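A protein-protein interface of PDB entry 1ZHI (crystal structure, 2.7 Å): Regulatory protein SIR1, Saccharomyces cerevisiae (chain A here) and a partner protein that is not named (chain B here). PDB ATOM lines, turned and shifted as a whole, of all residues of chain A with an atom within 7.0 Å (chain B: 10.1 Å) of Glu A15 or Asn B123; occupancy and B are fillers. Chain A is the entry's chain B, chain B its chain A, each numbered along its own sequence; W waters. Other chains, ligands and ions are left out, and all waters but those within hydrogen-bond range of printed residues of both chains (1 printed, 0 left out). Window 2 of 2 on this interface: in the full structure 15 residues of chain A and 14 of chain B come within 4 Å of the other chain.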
ATOM      1  N   GLU A  14      -7.673  11.491 -18.965  1.00  0.00           N
ATOM      2  CA  GLU A  14      -6.251  11.262 -18.575  1.00  0.00           C
ATOM      3  C   GLU A  14      -5.960  11.851 -17.184  1.00  0.00           C
ATOM      4  O   GLU A  14      -5.898  13.080 -16.999  1.00  0.00           O
ATOM      5  CB  GLU A  14      -5.282  11.835 -19.632  1.00  0.00           C
ATOM      6  CG  GLU A  14      -4.427  10.776 -20.341  1.00  0.00           C
ATOM      7  CD  GLU A  14      -3.138  11.329 -20.977  1.00  0.00           C
ATOM      8  OE1 GLU A  14      -2.494  12.242 -20.393  1.00  0.00           O
ATOM      9  OE2 GLU A  14      -2.753  10.830 -22.068  1.00  0.00           O
ATOM     10  N   GLU A  15      -5.798  10.971 -16.204  1.00  0.00           N
ATOM     11  CA  GLU A  15      -5.427  11.406 -14.864  1.00  0.00           C
ATOM     12  C   GLU A  15      -4.319  10.533 -14.280  1.00  0.00           C
ATOM     13  O   GLU A  15      -4.456   9.308 -14.194  1.00  0.00           O
ATOM     14  CB  GLU A  15      -6.654  11.439 -13.947  1.00  0.00           C
ATOM     15  CG  GLU A  15      -6.447  12.198 -12.653  1.00  0.00           C
ATOM     16  CD  GLU A  15      -6.902  13.642 -12.723  1.00  0.00           C
ATOM     17  OE1 GLU A  15      -7.155  14.160 -13.821  1.00  0.00           O
ATOM     18  OE2 GLU A  15      -7.014  14.261 -11.658  1.00  0.00           O
ATOM     19  N   TYR A  16      -3.212  11.182 -13.925  1.00  0.00           N
ATOM     20  CA  TYR A  16      -2.067  10.535 -13.292  1.00  0.00           C
ATOM     21  C   TYR A  16      -2.242  10.565 -11.793  1.00  0.00           C
ATOM     22  O   TYR A  16      -1.792  11.488 -11.131  1.00  0.00           O
ATOM     23  CB  TYR A  16      -0.786  11.280 -13.642  1.00  0.00           C
ATOM     24  CG  TYR A  16      -0.161  10.895 -14.957  1.00  0.00           C
ATOM     25  CD1 TYR A  16      -0.564  11.492 -16.145  1.00  0.00           C
ATOM     26  CD2 TYR A  16       0.859   9.954 -15.007  1.00  0.00           C
ATOM     27  CE1 TYR A  16       0.024  11.150 -17.342  1.00  0.00           C
ATOM     28  CE2 TYR A  16       1.454   9.608 -16.200  1.00  0.00           C
ATOM     29  CZ  TYR A  16       1.037  10.200 -17.361  1.00  0.00           C
ATOM     30  OH  TYR A  16       1.641   9.843 -18.548  1.00  0.00           O
ATOM     31  N   VAL A  17      -2.886   9.545 -11.257  1.00  0.00           N
ATOM     32  CA  VAL A  17      -3.276   9.556  -9.864  1.00  0.00           C
ATOM     33  C   VAL A  17      -2.066   9.333  -8.947  1.00  0.00           C
ATOM     34  O   VAL A  17      -2.099   9.681  -7.760  1.00  0.00           O
ATOM     35  CB  VAL A  17      -4.473   8.562  -9.580  1.00  0.00           C
ATOM     36  CG1 VAL A  17      -5.607   8.800 -10.574  1.00  0.00           C
ATOM     37  CG2 VAL A  17      -4.033   7.101  -9.626  1.00  0.00           C
ATOM     38  N   SER A  18      -1.004   8.761  -9.510  1.00  0.00           N
ATOM     39  CA  SER A  18       0.321   8.732  -8.879  1.00  0.00           C
ATOM     40  C   SER A  18       1.327   8.660 -10.017  1.00  0.00           C
ATOM     41  O   SER A  18       0.913   8.594 -11.177  1.00  0.00           O
ATOM     42  CB  SER A  18       0.452   7.532  -7.931  1.00  0.00           C
ATOM     43  OG  SER A  18       0.282   6.291  -8.609  1.00  0.00           O
ATOM     44  N   PHE A  21       0.542   5.229 -11.687  1.00  0.00           N
ATOM     45  CA  PHE A  21      -0.793   4.863 -12.127  1.00  0.00           C
ATOM     46  C   PHE A  21      -1.495   5.926 -12.936  1.00  0.00           C
ATOM     47  O   PHE A  21      -1.682   7.067 -12.484  1.00  0.00           O
ATOM     48  CB  PHE A  21      -1.647   4.395 -10.948  1.00  0.00           C
ATOM     49  CG  PHE A  21      -1.210   3.069 -10.392  1.00  0.00           C
ATOM     50  CD1 PHE A  21      -0.686   2.976  -9.096  1.00  0.00           C
ATOM     51  CD2 PHE A  21      -1.280   1.906 -11.185  1.00  0.00           C
ATOM     52  CE1 PHE A  21      -0.259   1.763  -8.594  1.00  0.00           C
ATOM     53  CE2 PHE A  21      -0.858   0.680 -10.676  1.00  0.00           C
ATOM     54  CZ  PHE A  21      -0.340   0.608  -9.377  1.00  0.00           C
ATOM     55  N   LEU A  22      -1.873   5.530 -14.150  1.00  0.00           N
ATOM     56  CA  LEU A  22      -2.527   6.404 -15.100  1.00  0.00           C
ATOM     57  C   LEU A  22      -3.939   5.923 -15.261  1.00  0.00           C
ATOM     58  O   LEU A  22      -4.167   4.738 -15.505  1.00  0.00           O
ATOM     59  CB  LEU A  22      -1.818   6.332 -16.457  1.00  0.00           C
ATOM     60  CG  LEU A  22      -1.846   7.479 -17.473  1.00  0.00           C
ATOM     61  CD1 LEU A  22      -1.437   6.948 -18.801  1.00  0.00           C
ATOM     62  CD2 LEU A  22      -3.184   8.150 -17.596  1.00  0.00           C
ATOM     63  N   VAL A  23      -4.891   6.839 -15.115  1.00  0.00           N
ATOM     64  CA  VAL A  23      -6.272   6.561 -15.510  1.00  0.00           C
ATOM     65  C   VAL A  23      -6.589   7.235 -16.836  1.00  0.00           C
ATOM     66  O   VAL A  23      -6.446   8.449 -16.972  1.00  0.00           O
ATOM     67  CB  VAL A  23      -7.297   6.999 -14.435  1.00  0.00           C
ATOM     68  CG1 VAL A  23      -8.719   6.776 -14.946  1.00  0.00           C
ATOM     69  CG2 VAL A  23      -7.072   6.237 -13.138  1.00  0.00           C
ATOM     70  N   ALA A  24      -7.020   6.437 -17.801  1.00  0.00           N
ATOM     71  CA  ALA A  24      -7.327   6.923 -19.138  1.00  0.00           C
ATOM     72  C   ALA A  24      -8.264   5.966 -19.872  1.00  0.00           C
ATOM     73  O   ALA A  24      -8.066   4.749 -19.845  1.00  0.00           O
ATOM     74  CB  ALA A  24      -6.055   7.105 -19.925  1.00  0.00           C
ATOM     75  N   PHE A  27      -9.681   2.988 -18.079  1.00  0.00           N
ATOM     76  CA  PHE A  27      -8.747   1.941 -17.652  1.00  0.00           C
ATOM     77  C   PHE A  27      -7.721   2.454 -16.655  1.00  0.00           C
ATOM     78  O   PHE A  27      -7.327   3.627 -16.690  1.00  0.00           O
ATOM     79  CB  PHE A  27      -8.062   1.289 -18.855  1.00  0.00           C
ATOM     80  CG  PHE A  27      -8.919   0.283 -19.547  1.00  0.00           C
ATOM     81  CD1 PHE A  27      -9.819   0.680 -20.530  1.00  0.00           C
ATOM     82  CD2 PHE A  27      -8.868  -1.056 -19.184  1.00  0.00           C
ATOM     83  CE1 PHE A  27     -10.642  -0.239 -21.157  1.00  0.00           C
ATOM     84  CE2 PHE A  27      -9.685  -1.986 -19.791  1.00  0.00           C
ATOM     85  CZ  PHE A  27     -10.579  -1.574 -20.793  1.00  0.00           C
ATOM     86  N   LEU A  28      -7.317   1.578 -15.745  1.00  0.00           N
ATOM     87  CA  LEU A  28      -6.216   1.875 -14.853  1.00  0.00           C
ATOM     88  C   LEU A  28      -4.979   1.261 -15.457  1.00  0.00           C
ATOM     89  O   LEU A  28      -4.937   0.051 -15.670  1.00  0.00           O
ATOM     90  CB  LEU A  28      -6.476   1.289 -13.455  1.00  0.00           C
ATOM     91  CG  LEU A  28      -5.490   1.670 -12.348  1.00  0.00           C
ATOM     92  CD1 LEU A  28      -5.406   3.176 -12.197  1.00  0.00           C
ATOM     93  CD2 LEU A  28      -5.874   1.014 -11.052  1.00  0.00           C
ATOM     94  N   HIS A  51      -5.729   9.095  -0.725  1.00  0.00           N
ATOM     95  CA  HIS A  51      -6.184  10.121  -1.659  1.00  0.00           C
ATOM     96  C   HIS A  51      -6.193   9.620  -3.105  1.00  0.00           C
ATOM     97  O   HIS A  51      -7.012  10.070  -3.924  1.00  0.00           O
ATOM     98  CB  HIS A  51      -5.362  11.414  -1.513  1.00  0.00           C
ATOM     99  CG  HIS A  51      -3.921  11.277  -1.915  1.00  0.00           C
ATOM    100  ND1 HIS A  51      -2.924  10.929  -1.022  1.00  0.00           N
ATOM    101  CD2 HIS A  51      -3.307  11.475  -3.108  1.00  0.00           C
ATOM    102  CE1 HIS A  51      -1.762  10.894  -1.656  1.00  0.00           C
ATOM    103  NE2 HIS A  51      -1.966  11.230  -2.919  1.00  0.00           N
ATOM    104  N   GLN A  52      -5.313   8.658  -3.397  1.00  0.00           N
ATOM    105  CA  GLN A  52      -5.236   8.058  -4.730  1.00  0.00           C
ATOM    106  C   GLN A  52      -6.342   7.024  -4.970  1.00  0.00           C
ATOM    107  O   GLN A  52      -6.894   6.943  -6.079  1.00  0.00           O
ATOM    108  CB  GLN A  52      -3.865   7.440  -4.972  1.00  0.00           C
ATOM    109  CG  GLN A  52      -2.706   8.400  -4.742  1.00  0.00           C
ATOM    110  CD  GLN A  52      -1.368   7.690  -4.623  1.00  0.00           C
ATOM    111  OE1 GLN A  52      -1.317   6.498  -4.290  1.00  0.00           O
ATOM    112  NE2 GLN A  52      -0.291   8.401  -4.916  1.00  0.00           N
ATOM    113  N   MET A  55      -9.494   9.053  -5.506  1.00  0.00           N
ATOM    114  CA  MET A  55      -9.571   9.587  -6.868  1.00  0.00           C
ATOM    115  C   MET A  55     -10.131   8.575  -7.827  1.00  0.00           C
ATOM    116  O   MET A  55     -10.943   8.909  -8.684  1.00  0.00           O
ATOM    117  CB  MET A  55      -8.201  10.050  -7.358  1.00  0.00           C
ATOM    118  CG  MET A  55      -7.800  11.429  -6.835  1.00  0.00           C
ATOM    119  SD  MET A  55      -6.178  12.002  -7.436  1.00  0.00           S
ATOM    120  CE  MET A  55      -5.081  11.519  -6.156  1.00  0.00           C
ATOM    121  N   MET A  59     -13.980   7.935 -10.211  1.00  0.00           N
ATOM    122  CA  MET A  59     -13.475   8.056 -11.562  1.00  0.00           C
ATOM    123  C   MET A  59     -14.235   7.272 -12.622  1.00  0.00           C
ATOM    124  O   MET A  59     -14.060   7.533 -13.816  1.00  0.00           O
ATOM    125  CB  MET A  59     -11.986   7.720 -11.608  1.00  0.00           C
ATOM    126  CG  MET A  59     -11.238   8.345 -12.780  1.00  0.00           C
ATOM    127  SD  MET A  59     -10.091   9.657 -12.313  1.00  0.00           S
ATOM    128  CE  MET A  59      -9.052   8.800 -11.195  1.00  0.00           C
ATOM    129  N   PRO B 104       7.149  13.069  -6.232  1.00  0.00           N
ATOM    130  CA  PRO B 104       7.382  14.009  -7.343  1.00  0.00           C
ATOM    131  C   PRO B 104       7.239  15.452  -6.925  1.00  0.00           C
ATOM    132  O   PRO B 104       7.841  16.332  -7.549  1.00  0.00           O
ATOM    133  CB  PRO B 104       6.312  13.628  -8.364  1.00  0.00           C
ATOM    134  CG  PRO B 104       5.274  12.906  -7.582  1.00  0.00           C
ATOM    135  CD  PRO B 104       5.930  12.262  -6.418  1.00  0.00           C
ATOM    136  N   LEU B 105       6.461  15.687  -5.876  1.00  0.00           N
ATOM    137  CA  LEU B 105       6.322  17.020  -5.306  1.00  0.00           C
ATOM    138  C   LEU B 105       7.559  17.398  -4.504  1.00  0.00           C
ATOM    139  O   LEU B 105       8.110  18.482  -4.680  1.00  0.00           O
ATOM    140  CB  LEU B 105       5.089  17.094  -4.425  1.00  0.00           C
ATOM    141  CG  LEU B 105       3.985  17.995  -4.966  1.00  0.00           C
ATOM    142  CD1 LEU B 105       2.615  17.391  -4.683  1.00  0.00           C
ATOM    143  CD2 LEU B 105       4.087  19.418  -4.394  1.00  0.00           C
ATOM    144  N   ASN B 119       1.475  26.335  -7.169  1.00  0.00           N
ATOM    145  CA  ASN B 119       0.108  26.711  -7.564  1.00  0.00           C
ATOM    146  C   ASN B 119      -0.530  25.713  -8.541  1.00  0.00           C
ATOM    147  O   ASN B 119      -1.563  25.999  -9.145  1.00  0.00           O
ATOM    148  CB  ASN B 119       0.050  28.156  -8.138  1.00  0.00           C
ATOM    149  CG  ASN B 119       0.868  28.330  -9.435  1.00  0.00           C
ATOM    150  OD1 ASN B 119       1.787  29.154  -9.493  1.00  0.00           O
ATOM    151  ND2 ASN B 119       0.508  27.577 -10.480  1.00  0.00           N
ATOM    152  N   ARG B 120       0.096  24.549  -8.688  1.00  0.00           N
ATOM    153  CA  ARG B 120      -0.374  23.517  -9.617  1.00  0.00           C
ATOM    154  C   ARG B 120      -1.162  22.421  -8.878  1.00  0.00           C
ATOM    155  O   ARG B 120      -1.071  22.320  -7.654  1.00  0.00           O
ATOM    156  CB  ARG B 120       0.818  22.905 -10.365  1.00  0.00           C
ATOM    157  CG  ARG B 120       1.348  23.755 -11.509  1.00  0.00           C
ATOM    158  CD  ARG B 120       2.815  24.123 -11.379  1.00  0.00           C
ATOM    159  NE  ARG B 120       3.184  25.260 -12.225  1.00  0.00           N
ATOM    160  CZ  ARG B 120       4.343  25.370 -12.876  1.00  0.00           C
ATOM    161  NH1 ARG B 120       5.256  24.409 -12.789  1.00  0.00           N
ATOM    162  NH2 ARG B 120       4.588  26.443 -13.621  1.00  0.00           N
ATOM    163  N   PRO B 121      -1.931  21.619  -9.598  1.00  0.00           N
ATOM    164  CA  PRO B 121      -2.587  20.439  -9.020  1.00  0.00           C
ATOM    165  C   PRO B 121      -1.565  19.356  -8.706  1.00  0.00           C
ATOM    166  O   PRO B 121      -0.537  19.278  -9.378  1.00  0.00           O
ATOM    167  CB  PRO B 121      -3.523  19.966 -10.141  1.00  0.00           C
ATOM    168  CG  PRO B 121      -3.549  21.045 -11.118  1.00  0.00           C
ATOM    169  CD  PRO B 121      -2.246  21.761 -11.026  1.00  0.00           C
ATOM    170  N   LEU B 122      -1.840  18.534  -7.700  1.00  0.00           N
ATOM    171  CA  LEU B 122      -0.904  17.482  -7.302  1.00  0.00           C
ATOM    172  C   LEU B 122      -0.647  16.454  -8.432  1.00  0.00           C
ATOM    173  O   LEU B 122       0.436  15.866  -8.510  1.00  0.00           O
ATOM    174  CB  LEU B 122      -1.366  16.810  -5.992  1.00  0.00           C
ATOM    175  CG  LEU B 122      -1.120  15.315  -5.748  1.00  0.00           C
ATOM    176  CD1 LEU B 122       0.279  15.025  -5.182  1.00  0.00           C
ATOM    177  CD2 LEU B 122      -2.203  14.755  -4.841  1.00  0.00           C
ATOM    178  N   ASN B 123      -1.631  16.278  -9.314  1.00  0.00           N
ATOM    179  CA  ASN B 123      -1.524  15.315 -10.401  1.00  0.00           C
ATOM    180  C   ASN B 123      -0.693  15.783 -11.575  1.00  0.00           C
ATOM    181  O   ASN B 123      -0.182  14.967 -12.348  1.00  0.00           O
ATOM    182  CB  ASN B 123      -2.907  14.885 -10.871  1.00  0.00           C
ATOM    183  CG  ASN B 123      -3.564  13.925  -9.910  1.00  0.00           C
ATOM    184  OD1 ASN B 123      -2.960  13.528  -8.909  1.00  0.00           O
ATOM    185  ND2 ASN B 123      -4.808  13.546 -10.198  1.00  0.00           N
ATOM    186  N   TYR B 124      -0.555  17.096 -11.711  1.00  0.00           N
ATOM    187  CA  TYR B 124       0.352  17.660 -12.694  1.00  0.00           C
ATOM    188  C   TYR B 124       1.787  17.240 -12.402  1.00  0.00           C
ATOM    189  O   TYR B 124       2.561  16.995 -13.325  1.00  0.00           O
ATOM    190  CB  TYR B 124       0.246  19.192 -12.736  1.00  0.00           C
ATOM    191  CG  TYR B 124       1.505  19.867 -13.240  1.00  0.00           C
ATOM    192  CD1 TYR B 124       1.761  19.987 -14.608  1.00  0.00           C
ATOM    193  CD2 TYR B 124       2.456  20.352 -12.348  1.00  0.00           C
ATOM    194  CE1 TYR B 124       2.923  20.592 -15.067  1.00  0.00           C
ATOM    195  CE2 TYR B 124       3.615  20.958 -12.795  1.00  0.00           C
ATOM    196  CZ  TYR B 124       3.843  21.078 -14.148  1.00  0.00           C
ATOM    197  OH  TYR B 124       5.000  21.682 -14.572  1.00  0.00           O
ATOM    198  N   TYR B 125       2.143  17.173 -11.120  1.00  0.00           N
ATOM    199  CA  TYR B 125       3.483  16.758 -10.722  1.00  0.00           C
ATOM    200  C   TYR B 125       3.732  15.295 -10.984  1.00  0.00           C
ATOM    201  O   TYR B 125       4.855  14.907 -11.269  1.00  0.00           O
ATOM    202  CB  TYR B 125       3.746  17.082  -9.260  1.00  0.00           C
ATOM    203  CG  TYR B 125       3.731  18.552  -8.970  1.00  0.00           C
ATOM    204  CD1 TYR B 125       2.638  19.141  -8.357  1.00  0.00           C
ATOM    205  CD2 TYR B 125       4.806  19.363  -9.326  1.00  0.00           C
ATOM    206  CE1 TYR B 125       2.614  20.513  -8.088  1.00  0.00           C
ATOM    207  CE2 TYR B 125       4.795  20.737  -9.062  1.00  0.00           C
ATOM    208  CZ  TYR B 125       3.696  21.300  -8.443  1.00  0.00           C
ATOM    209  OH  TYR B 125       3.665  22.650  -8.189  1.00  0.00           O
ATOM    210  N   ASN B 126       2.678  14.483 -10.897  1.00  0.00           N
ATOM    211  CA  ASN B 126       2.748  13.069 -11.269  1.00  0.00           C
ATOM    212  C   ASN B 126       2.995  12.884 -12.769  1.00  0.00           C
ATOM    213  O   ASN B 126       3.824  12.075 -13.165  1.00  0.00           O
ATOM    214  CB  ASN B 126       1.465  12.341 -10.874  1.00  0.00           C
ATOM    215  CG  ASN B 126       1.273  12.268  -9.384  1.00  0.00           C
ATOM    216  OD1 ASN B 126       2.241  12.148  -8.626  1.00  0.00           O
ATOM    217  ND2 ASN B 126       0.012  12.321  -8.947  1.00  0.00           N
ATOM    218  N   LYS B 127       2.259  13.631 -13.591  1.00  0.00           N
ATOM    219  CA  LYS B 127       2.435  13.597 -15.046  1.00  0.00           C
ATOM    220  C   LYS B 127       3.829  14.077 -15.459  1.00  0.00           C
ATOM    221  O   LYS B 127       4.481  13.441 -16.283  1.00  0.00           O
ATOM    222  CB  LYS B 127       1.353  14.425 -15.747  1.00  0.00           C
ATOM    223  CG  LYS B 127       1.417  14.407 -17.256  1.00  0.00           C
ATOM    224  CD  LYS B 127       0.522  15.485 -17.842  1.00  0.00           C
ATOM    225  CE  LYS B 127       0.167  15.208 -19.288  1.00  0.00           C
ATOM    226  NZ  LYS B 127      -1.278  14.875 -19.420  1.00  0.00           N
ATOM    227  N   LEU B 128       4.279  15.187 -14.868  1.00  0.00           N
ATOM    228  CA  LEU B 128       5.592  15.755 -15.165  1.00  0.00           C
ATOM    229  C   LEU B 128       6.726  14.792 -14.838  1.00  0.00           C
ATOM    230  O   LEU B 128       7.624  14.599 -15.660  1.00  0.00           O
ATOM    231  CB  LEU B 128       5.808  17.085 -14.434  1.00  0.00           C
ATOM    232  CG  LEU B 128       7.176  17.774 -14.627  1.00  0.00           C
ATOM    233  CD1 LEU B 128       7.363  18.293 -16.051  1.00  0.00           C
ATOM    234  CD2 LEU B 128       7.383  18.909 -13.621  1.00  0.00           C
ATOM    235  N   PHE B 129       6.701  14.189 -13.650  1.00  0.00           N
ATOM    236  CA  PHE B 129       7.767  13.256 -13.303  1.00  0.00           C
ATOM    237  C   PHE B 129       7.748  11.997 -14.171  1.00  0.00           C
ATOM    238  O   PHE B 129       8.747  11.648 -14.798  1.00  0.00           O
ATOM    239  CB  PHE B 129       7.797  12.908 -11.816  1.00  0.00           C
ATOM    240  CG  PHE B 129       9.155  12.462 -11.338  1.00  0.00           C
ATOM    241  CD1 PHE B 129      10.140  13.403 -11.019  1.00  0.00           C
ATOM    242  CD2 PHE B 129       9.470  11.109 -11.264  1.00  0.00           C
ATOM    243  CE1 PHE B 129      11.404  13.000 -10.599  1.00  0.00           C
ATOM    244  CE2 PHE B 129      10.727  10.695 -10.859  1.00  0.00           C
ATOM    245  CZ  PHE B 129      11.700  11.641 -10.519  1.00  0.00           C
ATOM    246  N   SER B 130       6.604  11.341 -14.233  1.00  0.00           N
ATOM    247  CA  SER B 130       6.455  10.162 -15.075  1.00  0.00           C
ATOM    248  C   SER B 130       6.920  10.395 -16.537  1.00  0.00           C
ATOM    249  O   SER B 130       7.445   9.481 -17.180  1.00  0.00           O
ATOM    250  CB  SER B 130       5.006   9.665 -15.033  1.00  0.00           C
ATOM    251  OG  SER B 130       4.684   8.932 -16.193  1.00  0.00           O
ATOM    252  N   GLU B 131       6.742  11.617 -17.033  1.00  0.00           N
ATOM    253  CA  GLU B 131       6.966  11.928 -18.449  1.00  0.00           C
ATOM    254  C   GLU B 131       8.400  12.359 -18.778  1.00  0.00           C
ATOM    255  O   GLU B 131       8.800  12.333 -19.942  1.00  0.00           O
ATOM    256  CB  GLU B 131       6.008  13.036 -18.906  1.00  0.00           C
ATOM    257  CG  GLU B 131       4.902  12.598 -19.851  1.00  0.00           C
ATOM    258  CD  GLU B 131       3.940  13.740 -20.211  1.00  0.00           C
ATOM    259  OE1 GLU B 131       4.371  14.923 -20.281  1.00  0.00           O
ATOM    260  OE2 GLU B 131       2.740  13.454 -20.421  1.00  0.00           O
HETATM  261  O   HOH W   1      -2.181  12.038  -7.120  1.00  0.00           O
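ND2 of Asn B123 is in hydrogen-bond range of OE2 of Glu A15 (2.7 Å).
O of Tyr A16 lies close to OD1 of Asn B123 (3.2 Å).
The side-chain amide nitrogen (ND2) of Asn B123 is in hydrogen-bond range of the side-chain sulfur (SD) of Met A55 (3.4 Å).
ND2 of Asn B126 sits at hydrogen-bond distance from O of Tyr A16, at 3.0 Å.
OE1 of Glu A14 is in salt-bridge range of NZ of Lys B127, at 3.1 Å.
OD1 of Asn B123 lies within hydrogen-bond range of ND2 of Asn B126.
O of Glu A15 sits at hydrogen-bond distance from N of Val A23, at 2.7 Å.
The side-chain hydroxyl of Ser A18 lies within hydrogen-bond range of the backbone NH of Phe A21 (3.3 Å).
Among the printed residues, pairs that only touch across the chains: Tyr A16 with Lys B127 (3.5 Å), Tyr A16 with Ser B130 (3.3 Å), Val A17 with Asn B126 (3.6 Å), Ser A18 with Asn B126 (3.6 Å) and His A51 with Leu B122 (3.9 Å).
Glu A15 touches just one residue of chain B: Asn B123.
Printed residues of chain B within 4 Å of Ser A18: Asn B126.
No residue of chain B comes within 4 Å of Leu A22.
No residue of chain B comes within 4 Å of Val A23.
Printed residues of chain B within 4 Å of His A51: Leu B122 (3.9 Å).
Of the printed residues of chain A, Leu B122 touches His A51 (3.9 Å).
Of chain A, only Glu A15 (2.7 Å), Tyr A16 (3.2 Å) and Met A55 (3.4 Å) come within 4 Å of Asn B123.
Of the printed residues of chain A, Lys B127 touches Glu A14 and Tyr A16.
Printed residues of chain A within 4 Å of Ser B130: Tyr A16.
The nearest residue of chain B that does not touch Glu A15 is Lys B127 (6.8 Å).
The nearest residue of chain A that does not touch Asn B123 is Val A17 (4.1 Å).
The nearest printed residue of chain A that does not touch Leu B122 is Met A55 (4.5 Å).
Hydrophobic or aromatic side chains of chain A within 4 Å of the printed part of chain B: Tyr A16, His A51 and Met A55.
Of the 15 printed residues of chain B, 5 touch a printed residue of chain A.
Among the printed residues, 10 pairs touch across the chains.
Among the printed residues, Asp or Glu carboxylates within 4 Å of a Lys or Arg side-chain nitrogen of the other chain: Glu A14 with Lys B127 (3.1 Å).
Water W1 lies within hydrogen-bond range of the backbone carbonyl oxygen (O) of Val A17 (2.4 Å), the side-chain amide oxygen (OD1) of Asn B123 (2.5 Å) and the side-chain amide nitrogen (ND2) of Asn B126 (2.9 Å).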
